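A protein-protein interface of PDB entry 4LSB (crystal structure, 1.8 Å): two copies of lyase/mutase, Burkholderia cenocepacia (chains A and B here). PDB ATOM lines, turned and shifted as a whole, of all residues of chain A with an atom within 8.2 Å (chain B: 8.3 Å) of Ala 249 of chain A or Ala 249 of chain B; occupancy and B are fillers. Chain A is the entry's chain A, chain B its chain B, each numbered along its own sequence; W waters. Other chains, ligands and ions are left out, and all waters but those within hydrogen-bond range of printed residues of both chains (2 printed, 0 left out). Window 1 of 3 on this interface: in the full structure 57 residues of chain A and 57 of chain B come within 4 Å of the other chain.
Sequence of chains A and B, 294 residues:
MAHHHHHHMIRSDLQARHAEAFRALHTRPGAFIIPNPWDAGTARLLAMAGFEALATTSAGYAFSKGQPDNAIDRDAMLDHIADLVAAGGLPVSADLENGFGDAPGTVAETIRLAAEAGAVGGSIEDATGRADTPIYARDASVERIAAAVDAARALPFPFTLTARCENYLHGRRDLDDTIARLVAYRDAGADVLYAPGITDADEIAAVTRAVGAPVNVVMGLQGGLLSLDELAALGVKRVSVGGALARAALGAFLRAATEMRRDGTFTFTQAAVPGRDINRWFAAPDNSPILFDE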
ATOM      1  N   TRP A  38     -14.336  18.113   0.404  1.00  0.00           N
ATOM      2  CA  TRP A  38     -15.776  17.850   0.298  1.00  0.00           C
ATOM      3  C   TRP A  38     -16.633  19.143   0.435  1.00  0.00           C
ATOM      4  O   TRP A  38     -17.865  19.066   0.384  1.00  0.00           O
ATOM      5  CB  TRP A  38     -16.177  16.783   1.324  1.00  0.00           C
ATOM      6  CG  TRP A  38     -16.009  17.235   2.706  1.00  0.00           C
ATOM      7  CD1 TRP A  38     -16.960  17.836   3.483  1.00  0.00           C
ATOM      8  CD2 TRP A  38     -14.817  17.191   3.492  1.00  0.00           C
ATOM      9  NE1 TRP A  38     -16.419  18.197   4.705  1.00  0.00           N
ATOM     10  CE2 TRP A  38     -15.097  17.818   4.722  1.00  0.00           C
ATOM     11  CE3 TRP A  38     -13.505  16.719   3.261  1.00  0.00           C
ATOM     12  CZ2 TRP A  38     -14.110  17.960   5.744  1.00  0.00           C
ATOM     13  CZ3 TRP A  38     -12.550  16.882   4.260  1.00  0.00           C
ATOM     14  CH2 TRP A  38     -12.861  17.475   5.479  1.00  0.00           C
ATOM     15  N   THR A  42     -12.689  23.363   2.598  1.00  0.00           N
ATOM     16  CA  THR A  42     -11.643  22.356   2.592  1.00  0.00           C
ATOM     17  C   THR A  42     -10.886  22.496   1.247  1.00  0.00           C
ATOM     18  O   THR A  42      -9.675  22.305   1.195  1.00  0.00           O
ATOM     19  CB  THR A  42     -12.166  20.920   2.827  1.00  0.00           C
ATOM     20  OG1 THR A  42     -13.274  20.652   1.980  1.00  0.00           O
ATOM     21  CG2 THR A  42     -12.615  20.673   4.288  1.00  0.00           C
ATOM     22  N   LEU A  45      -8.439  25.496   1.697  1.00  0.00           N
ATOM     23  CA  LEU A  45      -7.343  25.105   2.599  1.00  0.00           C
ATOM     24  C   LEU A  45      -6.349  24.206   1.961  1.00  0.00           C
ATOM     25  O   LEU A  45      -5.141  24.384   2.165  1.00  0.00           O
ATOM     26  CB  LEU A  45      -7.900  24.457   3.886  1.00  0.00           C
ATOM     27  CG  LEU A  45      -8.753  25.409   4.737  1.00  0.00           C
ATOM     28  CD1 LEU A  45      -9.530  24.664   5.823  1.00  0.00           C
ATOM     29  CD2 LEU A  45      -7.920  26.543   5.323  1.00  0.00           C
ATOM     30  N   GLY A 243     -12.812   9.339   0.668  1.00  0.00           N
ATOM     31  CA  GLY A 243     -13.478  10.052   1.761  1.00  0.00           C
ATOM     32  C   GLY A 243     -12.699  10.107   3.075  1.00  0.00           C
ATOM     33  O   GLY A 243     -13.252  10.519   4.091  1.00  0.00           O
ATOM     34  N   ALA A 244     -11.427   9.720   3.090  1.00  0.00           N
ATOM     35  CA  ALA A 244     -10.710   9.624   4.372  1.00  0.00           C
ATOM     36  C   ALA A 244     -10.422  10.944   5.049  1.00  0.00           C
ATOM     37  O   ALA A 244     -10.378  11.005   6.290  1.00  0.00           O
ATOM     38  CB  ALA A 244      -9.424   8.799   4.220  1.00  0.00           C
ATOM     39  N   LEU A 245     -10.263  12.023   4.277  1.00  0.00           N
ATOM     40  CA  LEU A 245     -10.134  13.343   4.883  1.00  0.00           C
ATOM     41  C   LEU A 245     -11.426  13.776   5.549  1.00  0.00           C
ATOM     42  O   LEU A 245     -11.350  14.325   6.679  1.00  0.00           O
ATOM     43  CB  LEU A 245      -9.625  14.441   3.919  1.00  0.00           C
ATOM     44  CG  LEU A 245      -8.135  14.612   3.672  1.00  0.00           C
ATOM     45  CD1 LEU A 245      -7.903  15.559   2.496  1.00  0.00           C
ATOM     46  CD2 LEU A 245      -7.401  15.132   4.892  1.00  0.00           C
ATOM     47  N   ALA A 246     -12.575  13.572   4.875  1.00  0.00           N
ATOM     48  CA  ALA A 246     -13.914  13.813   5.468  1.00  0.00           C
ATOM     49  C   ALA A 246     -14.090  13.001   6.728  1.00  0.00           C
ATOM     50  O   ALA A 246     -14.558  13.472   7.749  1.00  0.00           O
ATOM     51  CB  ALA A 246     -15.025  13.461   4.489  1.00  0.00           C
ATOM     52  N   ARG A 247     -13.696  11.754   6.648  1.00  0.00           N
ATOM     53  CA  ARG A 247     -13.821  10.871   7.777  1.00  0.00           C
ATOM     54  C   ARG A 247     -12.894  11.215   8.907  1.00  0.00           C
ATOM     55  O   ARG A 247     -13.237  10.963  10.079  1.00  0.00           O
ATOM     56  CB  ARG A 247     -13.701   9.403   7.337  1.00  0.00           C
ATOM     57  CG  ARG A 247     -14.971   8.956   6.591  1.00  0.00           C
ATOM     58  CD  ARG A 247     -15.049   7.476   6.214  1.00  0.00           C
ATOM     59  NE  ARG A 247     -13.972   7.073   5.265  1.00  0.00           N
ATOM     60  CZ  ARG A 247     -12.816   6.506   5.600  1.00  0.00           C
ATOM     61  NH1 ARG A 247     -12.524   6.257   6.862  1.00  0.00           N
ATOM     62  NH2 ARG A 247     -11.928   6.191   4.657  1.00  0.00           N
ATOM     63  N   ALA A 248     -11.697  11.711   8.590  1.00  0.00           N
ATOM     64  CA  ALA A 248     -10.843  12.267   9.622  1.00  0.00           C
ATOM     65  C   ALA A 248     -11.500  13.405  10.356  1.00  0.00           C
ATOM     66  O   ALA A 248     -11.508  13.455  11.590  1.00  0.00           O
ATOM     67  CB  ALA A 248      -9.535  12.732   9.039  1.00  0.00           C
ATOM     68  N   ALA A 249     -11.993  14.367   9.586  1.00  0.00           N
ATOM     69  CA  ALA A 249     -12.667  15.526  10.135  1.00  0.00           C
ATOM     70  C   ALA A 249     -13.787  15.104  11.005  1.00  0.00           C
ATOM     71  O   ALA A 249     -13.942  15.590  12.160  1.00  0.00           O
ATOM     72  CB  ALA A 249     -13.171  16.406   9.013  1.00  0.00           C
ATOM     73  N   LEU A 250     -14.587  14.187  10.475  1.00  0.00           N
ATOM     74  CA  LEU A 250     -15.683  13.603  11.238  1.00  0.00           C
ATOM     75  C   LEU A 250     -15.239  12.795  12.473  1.00  0.00           C
ATOM     76  O   LEU A 250     -15.865  12.864  13.532  1.00  0.00           O
ATOM     77  CB  LEU A 250     -16.590  12.780  10.333  1.00  0.00           C
ATOM     78  CG  LEU A 250     -17.393  13.630   9.338  1.00  0.00           C
ATOM     79  CD1 LEU A 250     -18.194  12.690   8.455  1.00  0.00           C
ATOM     80  CD2 LEU A 250     -18.327  14.647  10.031  1.00  0.00           C
ATOM     81  N   GLY A 251     -14.113  12.121  12.382  1.00  0.00           N
ATOM     82  CA  GLY A 251     -13.577  11.512  13.597  1.00  0.00           C
ATOM     83  C   GLY A 251     -13.358  12.500  14.754  1.00  0.00           C
ATOM     84  O   GLY A 251     -13.688  12.214  15.912  1.00  0.00           O
ATOM     85  N   ALA A 252     -12.771  13.652  14.452  1.00  0.00           N
ATOM     86  CA  ALA A 252     -12.517  14.655  15.459  1.00  0.00           C
ATOM     87  C   ALA A 252     -13.814  15.230  15.983  1.00  0.00           C
ATOM     88  O   ALA A 252     -13.971  15.481  17.181  1.00  0.00           O
ATOM     89  CB  ALA A 252     -11.660  15.767  14.912  1.00  0.00           C
ATOM     90  N   PHE A 253     -14.732  15.457  15.066  1.00  0.00           N
ATOM     91  CA  PHE A 253     -16.069  15.932  15.416  1.00  0.00           C
ATOM     92  C   PHE A 253     -16.738  14.970  16.380  1.00  0.00           C
ATOM     93  O   PHE A 253     -17.303  15.379  17.443  1.00  0.00           O
ATOM     94  CB  PHE A 253     -16.874  16.086  14.144  1.00  0.00           C
ATOM     95  CG  PHE A 253     -18.284  16.438  14.380  1.00  0.00           C
ATOM     96  CD1 PHE A 253     -18.637  17.765  14.612  1.00  0.00           C
ATOM     97  CD2 PHE A 253     -19.251  15.481  14.401  1.00  0.00           C
ATOM     98  CE1 PHE A 253     -19.940  18.124  14.805  1.00  0.00           C
ATOM     99  CE2 PHE A 253     -20.577  15.834  14.651  1.00  0.00           C
ATOM    100  CZ  PHE A 253     -20.902  17.139  14.869  1.00  0.00           C
ATOM    101  N   LEU A 254     -16.654  13.683  16.074  1.00  0.00           N
ATOM    102  CA  LEU A 254     -17.251  12.677  16.951  1.00  0.00           C
ATOM    103  C   LEU A 254     -16.577  12.529  18.308  1.00  0.00           C
ATOM    104  O   LEU A 254     -17.259  12.265  19.320  1.00  0.00           O
ATOM    105  CB  LEU A 254     -17.364  11.312  16.276  1.00  0.00           C
ATOM    106  CG  LEU A 254     -18.519  11.161  15.244  1.00  0.00           C
ATOM    107  CD1 LEU A 254     -18.332   9.859  14.436  1.00  0.00           C
ATOM    108  CD2 LEU A 254     -19.889  11.139  15.867  1.00  0.00           C
ATOM    109  N   ARG A 255     -15.256  12.635  18.362  1.00  0.00           N
ATOM    110  CA  ARG A 255     -14.595  12.614  19.653  1.00  0.00           C
ATOM    111  C   ARG A 255     -15.013  13.808  20.517  1.00  0.00           C
ATOM    112  O   ARG A 255     -15.096  13.704  21.746  1.00  0.00           O
ATOM    113  CB  ARG A 255     -13.097  12.549  19.453  1.00  0.00           C
ATOM    114  CG  ARG A 255     -12.668  11.212  18.858  1.00  0.00           C
ATOM    115  CD  ARG A 255     -11.174  11.038  18.838  1.00  0.00           C
ATOM    116  NE  ARG A 255     -10.526  12.003  17.939  1.00  0.00           N
ATOM    117  CZ  ARG A 255     -10.291  11.803  16.639  1.00  0.00           C
ATOM    118  NH1 ARG A 255     -10.682  10.694  16.068  1.00  0.00           N
ATOM    119  NH2 ARG A 255      -9.640  12.710  15.907  1.00  0.00           N
ATOM    120  N   ALA A 256     -15.272  14.949  19.882  1.00  0.00           N
ATOM    121  CA  ALA A 256     -15.793  16.135  20.604  1.00  0.00           C
ATOM    122  C   ALA A 256     -17.202  15.920  21.098  1.00  0.00           C
ATOM    123  O   ALA A 256     -17.495  16.239  22.262  1.00  0.00           O
ATOM    124  CB  ALA A 256     -15.706  17.401  19.750  1.00  0.00           C
ATOM    125  N   PHE A 268     -11.782  19.497  23.772  1.00  0.00           N
ATOM    126  CA  PHE A 268     -11.520  19.342  22.335  1.00  0.00           C
ATOM    127  C   PHE A 268     -11.240  20.667  21.630  1.00  0.00           C
ATOM    128  O   PHE A 268     -10.661  20.674  20.547  1.00  0.00           O
ATOM    129  CB  PHE A 268     -12.690  18.666  21.631  1.00  0.00           C
ATOM    130  CG  PHE A 268     -13.896  19.504  21.558  1.00  0.00           C
ATOM    131  CD1 PHE A 268     -14.078  20.387  20.506  1.00  0.00           C
ATOM    132  CD2 PHE A 268     -14.861  19.411  22.530  1.00  0.00           C
ATOM    133  CE1 PHE A 268     -15.221  21.165  20.421  1.00  0.00           C
ATOM    134  CE2 PHE A 268     -16.019  20.180  22.457  1.00  0.00           C
ATOM    135  CZ  PHE A 268     -16.191  21.073  21.402  1.00  0.00           C
ATOM    136  N   ALA A 271      -7.382  21.845  20.624  1.00  0.00           N
ATOM    137  CA  ALA A 271      -6.777  21.380  19.371  1.00  0.00           C
ATOM    138  C   ALA A 271      -7.464  21.925  18.109  1.00  0.00           C
ATOM    139  O   ALA A 271      -7.026  21.648  16.975  1.00  0.00           O
ATOM    140  CB  ALA A 271      -6.818  19.862  19.355  1.00  0.00           C
ATOM    141  N   ALA A 272      -8.552  22.658  18.271  1.00  0.00           N
ATOM    142  CA  ALA A 272      -9.269  23.226  17.134  1.00  0.00           C
ATOM    143  C   ALA A 272      -8.463  24.335  16.522  1.00  0.00           C
ATOM    144  O   ALA A 272      -7.608  24.936  17.191  1.00  0.00           O
ATOM    145  CB  ALA A 272     -10.612  23.782  17.582  1.00  0.00           C
ATOM    146  N   VAL A 273      -8.716  24.645  15.251  1.00  0.00           N
ATOM    147  CA  VAL A 273      -8.068  25.799  14.640  1.00  0.00           C
ATOM    148  C   VAL A 273      -8.642  27.040  15.299  1.00  0.00           C
ATOM    149  O   VAL A 273      -9.840  27.132  15.480  1.00  0.00           O
ATOM    150  CB  VAL A 273      -8.210  25.810  13.094  1.00  0.00           C
ATOM    151  CG1 VAL A 273      -9.665  25.964  12.675  1.00  0.00           C
ATOM    152  CG2 VAL A 273      -7.343  26.902  12.476  1.00  0.00           C
ATOM    153  N   TRP B  38     -22.967  22.143  11.267  1.00  0.00           N
ATOM    154  CA  TRP B  38     -22.906  23.086  10.154  1.00  0.00           C
ATOM    155  C   TRP B  38     -23.310  22.455   8.810  1.00  0.00           C
ATOM    156  O   TRP B  38     -23.284  23.125   7.789  1.00  0.00           O
ATOM    157  CB  TRP B  38     -21.484  23.733  10.024  1.00  0.00           C
ATOM    158  CG  TRP B  38     -20.433  22.723   9.722  1.00  0.00           C
ATOM    159  CD1 TRP B  38     -19.971  22.360   8.480  1.00  0.00           C
ATOM    160  CD2 TRP B  38     -19.784  21.873  10.653  1.00  0.00           C
ATOM    161  NE1 TRP B  38     -19.031  21.366   8.605  1.00  0.00           N
ATOM    162  CE2 TRP B  38     -18.879  21.077   9.932  1.00  0.00           C
ATOM    163  CE3 TRP B  38     -19.776  21.794  12.051  1.00  0.00           C
ATOM    164  CZ2 TRP B  38     -18.039  20.139  10.565  1.00  0.00           C
ATOM    165  CZ3 TRP B  38     -18.966  20.822  12.654  1.00  0.00           C
ATOM    166  CH2 TRP B  38     -18.121  20.044  11.924  1.00  0.00           C
ATOM    167  N   THR B  42     -23.404  16.386  10.147  1.00  0.00           N
ATOM    168  CA  THR B  42     -23.105  16.682  11.518  1.00  0.00           C
ATOM    169  C   THR B  42     -24.370  16.762  12.346  1.00  0.00           C
ATOM    170  O   THR B  42     -24.356  16.353  13.479  1.00  0.00           O
ATOM    171  CB  THR B  42     -22.194  17.940  11.654  1.00  0.00           C
ATOM    172  OG1 THR B  42     -22.735  19.048  10.918  1.00  0.00           O
ATOM    173  CG2 THR B  42     -20.808  17.649  11.180  1.00  0.00           C
ATOM    174  N   LEU B  45     -25.313  13.213  13.118  1.00  0.00           N
ATOM    175  CA  LEU B  45     -24.416  12.581  14.069  1.00  0.00           C
ATOM    176  C   LEU B  45     -24.670  13.091  15.472  1.00  0.00           C
ATOM    177  O   LEU B  45     -24.640  12.337  16.429  1.00  0.00           O
ATOM    178  CB  LEU B  45     -22.977  12.826  13.701  1.00  0.00           C
ATOM    179  CG  LEU B  45     -22.569  12.099  12.389  1.00  0.00           C
ATOM    180  CD1 LEU B  45     -21.215  12.605  11.939  1.00  0.00           C
ATOM    181  CD2 LEU B  45     -22.560  10.567  12.581  1.00  0.00           C
ATOM    182  N   GLY B 243     -18.887  28.117  16.582  1.00  0.00           N
ATOM    183  CA  GLY B 243     -18.165  27.411  15.477  1.00  0.00           C
ATOM    184  C   GLY B 243     -17.123  26.398  15.939  1.00  0.00           C
ATOM    185  O   GLY B 243     -16.332  25.937  15.117  1.00  0.00           O
ATOM    186  N   ALA B 244     -17.071  26.071  17.232  1.00  0.00           N
ATOM    187  CA  ALA B 244     -15.965  25.258  17.742  1.00  0.00           C
ATOM    188  C   ALA B 244     -15.938  23.849  17.262  1.00  0.00           C
ATOM    189  O   ALA B 244     -14.852  23.261  17.142  1.00  0.00           O
ATOM    190  CB  ALA B 244     -15.920  25.288  19.255  1.00  0.00           C
ATOM    191  N   LEU B 245     -17.105  23.260  17.023  1.00  0.00           N
ATOM    192  CA  LEU B 245     -17.107  21.924  16.430  1.00  0.00           C
ATOM    193  C   LEU B 245     -16.549  21.967  14.992  1.00  0.00           C
ATOM    194  O   LEU B 245     -15.738  21.093  14.601  1.00  0.00           O
ATOM    195  CB  LEU B 245     -18.468  21.269  16.480  1.00  0.00           C
ATOM    196  CG  LEU B 245     -18.890  20.821  17.863  1.00  0.00           C
ATOM    197  CD1 LEU B 245     -20.366  20.442  17.911  1.00  0.00           C
ATOM    198  CD2 LEU B 245     -17.965  19.690  18.330  1.00  0.00           C
ATOM    199  N   ALA B 246     -16.982  22.950  14.205  1.00  0.00           N
ATOM    200  CA  ALA B 246     -16.462  23.117  12.852  1.00  0.00           C
ATOM    201  C   ALA B 246     -14.946  23.334  12.903  1.00  0.00           C
ATOM    202  O   ALA B 246     -14.205  22.762  12.100  1.00  0.00           O
ATOM    203  CB  ALA B 246     -17.170  24.287  12.140  1.00  0.00           C
ATOM    204  N   ARG B 247     -14.468  24.094  13.882  1.00  0.00           N
ATOM    205  CA  ARG B 247     -13.056  24.358  14.011  1.00  0.00           C
ATOM    206  C   ARG B 247     -12.305  23.103  14.542  1.00  0.00           C
ATOM    207  O   ARG B 247     -11.178  22.883  14.200  1.00  0.00           O
ATOM    208  CB  ARG B 247     -12.790  25.639  14.835  1.00  0.00           C
ATOM    209  CG  ARG B 247     -13.271  26.916  14.174  1.00  0.00           C
ATOM    210  CD  ARG B 247     -12.840  28.189  14.914  1.00  0.00           C
ATOM    211  NE  ARG B 247     -13.535  28.300  16.221  1.00  0.00           N
ATOM    212  CZ  ARG B 247     -13.031  27.948  17.392  1.00  0.00           C
ATOM    213  NH1 ARG B 247     -11.790  27.508  17.504  1.00  0.00           N
ATOM    214  NH2 ARG B 247     -13.775  28.083  18.494  1.00  0.00           N
ATOM    215  N   ALA B 248     -12.932  22.279  15.366  1.00  0.00           N
ATOM    216  CA  ALA B 248     -12.330  21.013  15.722  1.00  0.00           C
ATOM    217  C   ALA B 248     -12.108  20.132  14.474  1.00  0.00           C
ATOM    218  O   ALA B 248     -11.035  19.513  14.281  1.00  0.00           O
ATOM    219  CB  ALA B 248     -13.174  20.305  16.742  1.00  0.00           C
ATOM    220  N   ALA B 249     -13.129  20.039  13.650  1.00  0.00           N
ATOM    221  CA  ALA B 249     -13.041  19.207  12.440  1.00  0.00           C
ATOM    222  C   ALA B 249     -11.895  19.739  11.536  1.00  0.00           C
ATOM    223  O   ALA B 249     -11.065  18.997  10.993  1.00  0.00           O
ATOM    224  CB  ALA B 249     -14.349  19.266  11.705  1.00  0.00           C
ATOM    225  N   LEU B 250     -11.873  21.052  11.398  1.00  0.00           N
ATOM    226  CA  LEU B 250     -10.878  21.697  10.568  1.00  0.00           C
ATOM    227  C   LEU B 250      -9.468  21.548  11.125  1.00  0.00           C
ATOM    228  O   LEU B 250      -8.540  21.359  10.360  1.00  0.00           O
ATOM    229  CB  LEU B 250     -11.272  23.139  10.296  1.00  0.00           C
ATOM    230  CG  LEU B 250     -12.495  23.246   9.388  1.00  0.00           C
ATOM    231  CD1 LEU B 250     -12.946  24.686   9.251  1.00  0.00           C
ATOM    232  CD2 LEU B 250     -12.212  22.701   7.988  1.00  0.00           C
ATOM    233  N   GLY B 251      -9.314  21.530  12.440  1.00  0.00           N
ATOM    234  CA  GLY B 251      -7.980  21.298  13.040  1.00  0.00           C
ATOM    235  C   GLY B 251      -7.512  19.911  12.659  1.00  0.00           C
ATOM    236  O   GLY B 251      -6.353  19.722  12.272  1.00  0.00           O
ATOM    237  N   ALA B 252      -8.420  18.940  12.658  1.00  0.00           N
ATOM    238  CA  ALA B 252      -7.981  17.582  12.308  1.00  0.00           C
ATOM    239  C   ALA B 252      -7.670  17.510  10.823  1.00  0.00           C
ATOM    240  O   ALA B 252      -6.658  16.917  10.373  1.00  0.00           O
ATOM    241  CB  ALA B 252      -9.032  16.571  12.671  1.00  0.00           C
ATOM    242  N   PHE B 253      -8.572  18.072  10.042  1.00  0.00           N
ATOM    243  CA  PHE B 253      -8.327  18.233   8.564  1.00  0.00           C
ATOM    244  C   PHE B 253      -6.964  18.863   8.268  1.00  0.00           C
ATOM    245  O   PHE B 253      -6.193  18.380   7.422  1.00  0.00           O
ATOM    246  CB  PHE B 253      -9.408  19.117   7.979  1.00  0.00           C
ATOM    247  CG  PHE B 253      -9.235  19.392   6.535  1.00  0.00           C
ATOM    248  CD1 PHE B 253      -9.579  18.431   5.606  1.00  0.00           C
ATOM    249  CD2 PHE B 253      -8.674  20.589   6.099  1.00  0.00           C
ATOM    250  CE1 PHE B 253      -9.423  18.665   4.263  1.00  0.00           C
ATOM    251  CE2 PHE B 253      -8.500  20.808   4.740  1.00  0.00           C
ATOM    252  CZ  PHE B 253      -8.896  19.862   3.840  1.00  0.00           C
ATOM    253  N   LEU B 254      -6.652  19.963   8.959  1.00  0.00           N
ATOM    254  CA  LEU B 254      -5.339  20.634   8.751  1.00  0.00           C
ATOM    255  C   LEU B 254      -4.172  19.789   9.195  1.00  0.00           C
ATOM    256  O   LEU B 254      -3.132  19.791   8.546  1.00  0.00           O
ATOM    257  CB  LEU B 254      -5.271  22.022   9.442  1.00  0.00           C
ATOM    258  CG  LEU B 254      -6.096  23.071   8.653  1.00  0.00           C
ATOM    259  CD1 LEU B 254      -6.254  24.426   9.385  1.00  0.00           C
ATOM    260  CD2 LEU B 254      -5.531  23.307   7.261  1.00  0.00           C
ATOM    261  N   ARG B 255      -4.310  19.065  10.311  1.00  0.00           N
ATOM    262  CA  ARG B 255      -3.202  18.191  10.704  1.00  0.00           C
ATOM    263  C   ARG B 255      -2.927  17.092   9.657  1.00  0.00           C
ATOM    264  O   ARG B 255      -1.763  16.742   9.389  1.00  0.00           O
ATOM    265  CB  ARG B 255      -3.418  17.618  12.067  1.00  0.00           C
ATOM    266  CG  ARG B 255      -3.279  18.663  13.169  1.00  0.00           C
ATOM    267  CD  ARG B 255      -3.415  18.024  14.540  1.00  0.00           C
ATOM    268  NE  ARG B 255      -4.765  17.590  14.867  1.00  0.00           N
ATOM    269  CZ  ARG B 255      -5.735  18.377  15.336  1.00  0.00           C
ATOM    270  NH1 ARG B 255      -5.575  19.686  15.488  1.00  0.00           N
ATOM    271  NH2 ARG B 255      -6.904  17.829  15.628  1.00  0.00           N
ATOM    272  N   ALA B 256      -3.988  16.611   9.040  1.00  0.00           N
ATOM    273  CA  ALA B 256      -3.857  15.605   7.966  1.00  0.00           C
ATOM    274  C   ALA B 256      -3.176  16.203   6.729  1.00  0.00           C
ATOM    275  O   ALA B 256      -2.266  15.572   6.143  1.00  0.00           O
ATOM    276  CB  ALA B 256      -5.208  15.065   7.591  1.00  0.00           C
ATOM    277  N   PHE B 268      -2.870   9.829   9.611  1.00  0.00           N
ATOM    278  CA  PHE B 268      -4.053  10.493  10.078  1.00  0.00           C
ATOM    279  C   PHE B 268      -5.365   9.663   9.895  1.00  0.00           C
ATOM    280  O   PHE B 268      -6.331   9.858  10.592  1.00  0.00           O
ATOM    281  CB  PHE B 268      -4.142  11.864   9.418  1.00  0.00           C
ATOM    282  CG  PHE B 268      -4.616  11.829   7.997  1.00  0.00           C
ATOM    283  CD1 PHE B 268      -5.970  11.660   7.697  1.00  0.00           C
ATOM    284  CD2 PHE B 268      -3.721  11.983   6.962  1.00  0.00           C
ATOM    285  CE1 PHE B 268      -6.407  11.687   6.406  1.00  0.00           C
ATOM    286  CE2 PHE B 268      -4.158  11.953   5.625  1.00  0.00           C
ATOM    287  CZ  PHE B 268      -5.507  11.835   5.364  1.00  0.00           C
ATOM    288  N   ALA B 271      -7.140   7.408  12.865  1.00  0.00           N
ATOM    289  CA  ALA B 271      -8.188   7.964  13.770  1.00  0.00           C
ATOM    290  C   ALA B 271      -9.513   8.373  13.102  1.00  0.00           C
ATOM    291  O   ALA B 271     -10.440   8.746  13.788  1.00  0.00           O
ATOM    292  CB  ALA B 271      -7.645   9.138  14.528  1.00  0.00           C
ATOM    293  N   ALA B 272      -9.611   8.287  11.796  1.00  0.00           N
ATOM    294  CA  ALA B 272     -10.833   8.613  11.083  1.00  0.00           C
ATOM    295  C   ALA B 272     -11.966   7.649  11.409  1.00  0.00           C
ATOM    296  O   ALA B 272     -11.754   6.497  11.745  1.00  0.00           O
ATOM    297  CB  ALA B 272     -10.575   8.587   9.578  1.00  0.00           C
ATOM    298  N   VAL B 273     -13.192   8.111  11.302  1.00  0.00           N
ATOM    299  CA  VAL B 273     -14.288   7.188  11.466  1.00  0.00           C
ATOM    300  C   VAL B 273     -14.262   6.184  10.296  1.00  0.00           C
ATOM    301  O   VAL B 273     -14.132   6.585   9.141  1.00  0.00           O
ATOM    302  CB  VAL B 273     -15.599   7.942  11.586  1.00  0.00           C
ATOM    303  CG1 VAL B 273     -15.835   8.817  10.359  1.00  0.00           C
ATOM    304  CG2 VAL B 273     -16.726   6.957  11.797  1.00  0.00           C
HETATM  305  O   HOH W   1      -9.674  12.038  13.155  1.00  0.00           O
HETATM  306  O   HOH W   2      -9.173  19.405  16.233  1.00  0.00           O
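Of the 21 printed residues of chain A, 15 touch a printed residue of chain B. Hydrophobic or aromatic side chains of chain B that line the printed part of chain A: Trp 38, Leu 45, Leu 245, Ala 248, Ala 249, Leu 250, Ala 252, Phe 253, Ala 256, Phe 268, Ala 271, Ala 272 and Val 273. Among the printed residues, 27 pairs touch across the chains. Among the printed residues, no Asp or Glu carboxylate lies within 4 Å of a Lys or Arg side-chain nitrogen of the other chain.
Positions printed for both chains: 38, 42, 45, 243, 244, 245, 246, 247, 248, 249, 250, 251, 252, 253, 254, 255, 256, 268, 271, 272 and 273.
The backbone NH (N) of Trp 38 of chain B sits at hydrogen-bond distance from the side-chain hydroxyl (OG1) of Thr 42 of chain B (3.1 Å).
O of Val 273 of chain B is in hydrogen-bond range of NH1 of Arg 247 of chain A (2.8 Å). O of Ala 271 of chain B lies within hydrogen-bond range of NH1 of Arg 255 of chain A, at 3.0 Å. O of Ala 271 of chain A is in hydrogen-bond range of NH1 of Arg 255 of chain B, 2.9 Å away. The backbone carbonyl oxygen of Val 273 of chain A is in hydrogen-bond range of the guanidinium group of Arg 247 of chain B (2.8 Å).
Water W1 lies within hydrogen-bond range of the backbone carbonyl oxygen of Ala 248 of chain A, the guanidinium group of Arg 255 of chain A and the backbone carbonyl oxygen of Ala 271 of chain B.
Ala 249 of chain A touches just one residue of chain B: Ala 249 (3.7 Å). Of the printed residues of chain A, Ala 249 of chain B touches Ala 249. Ala 248 of chain A touches two residues of chain B. Printed residues of chain A within 4 Å of Leu 250 of chain B: Leu 45. Ala 246 of chain B touches none of the printed residues of chain A. The nearest residue of chain A that does not touch Ala 249 of chain B is Ala 252 of chain A (4.5 Å). The nearest printed residue of chain A that does not touch Leu 245 of chain B is Ala 252 of chain A (5.9 Å).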
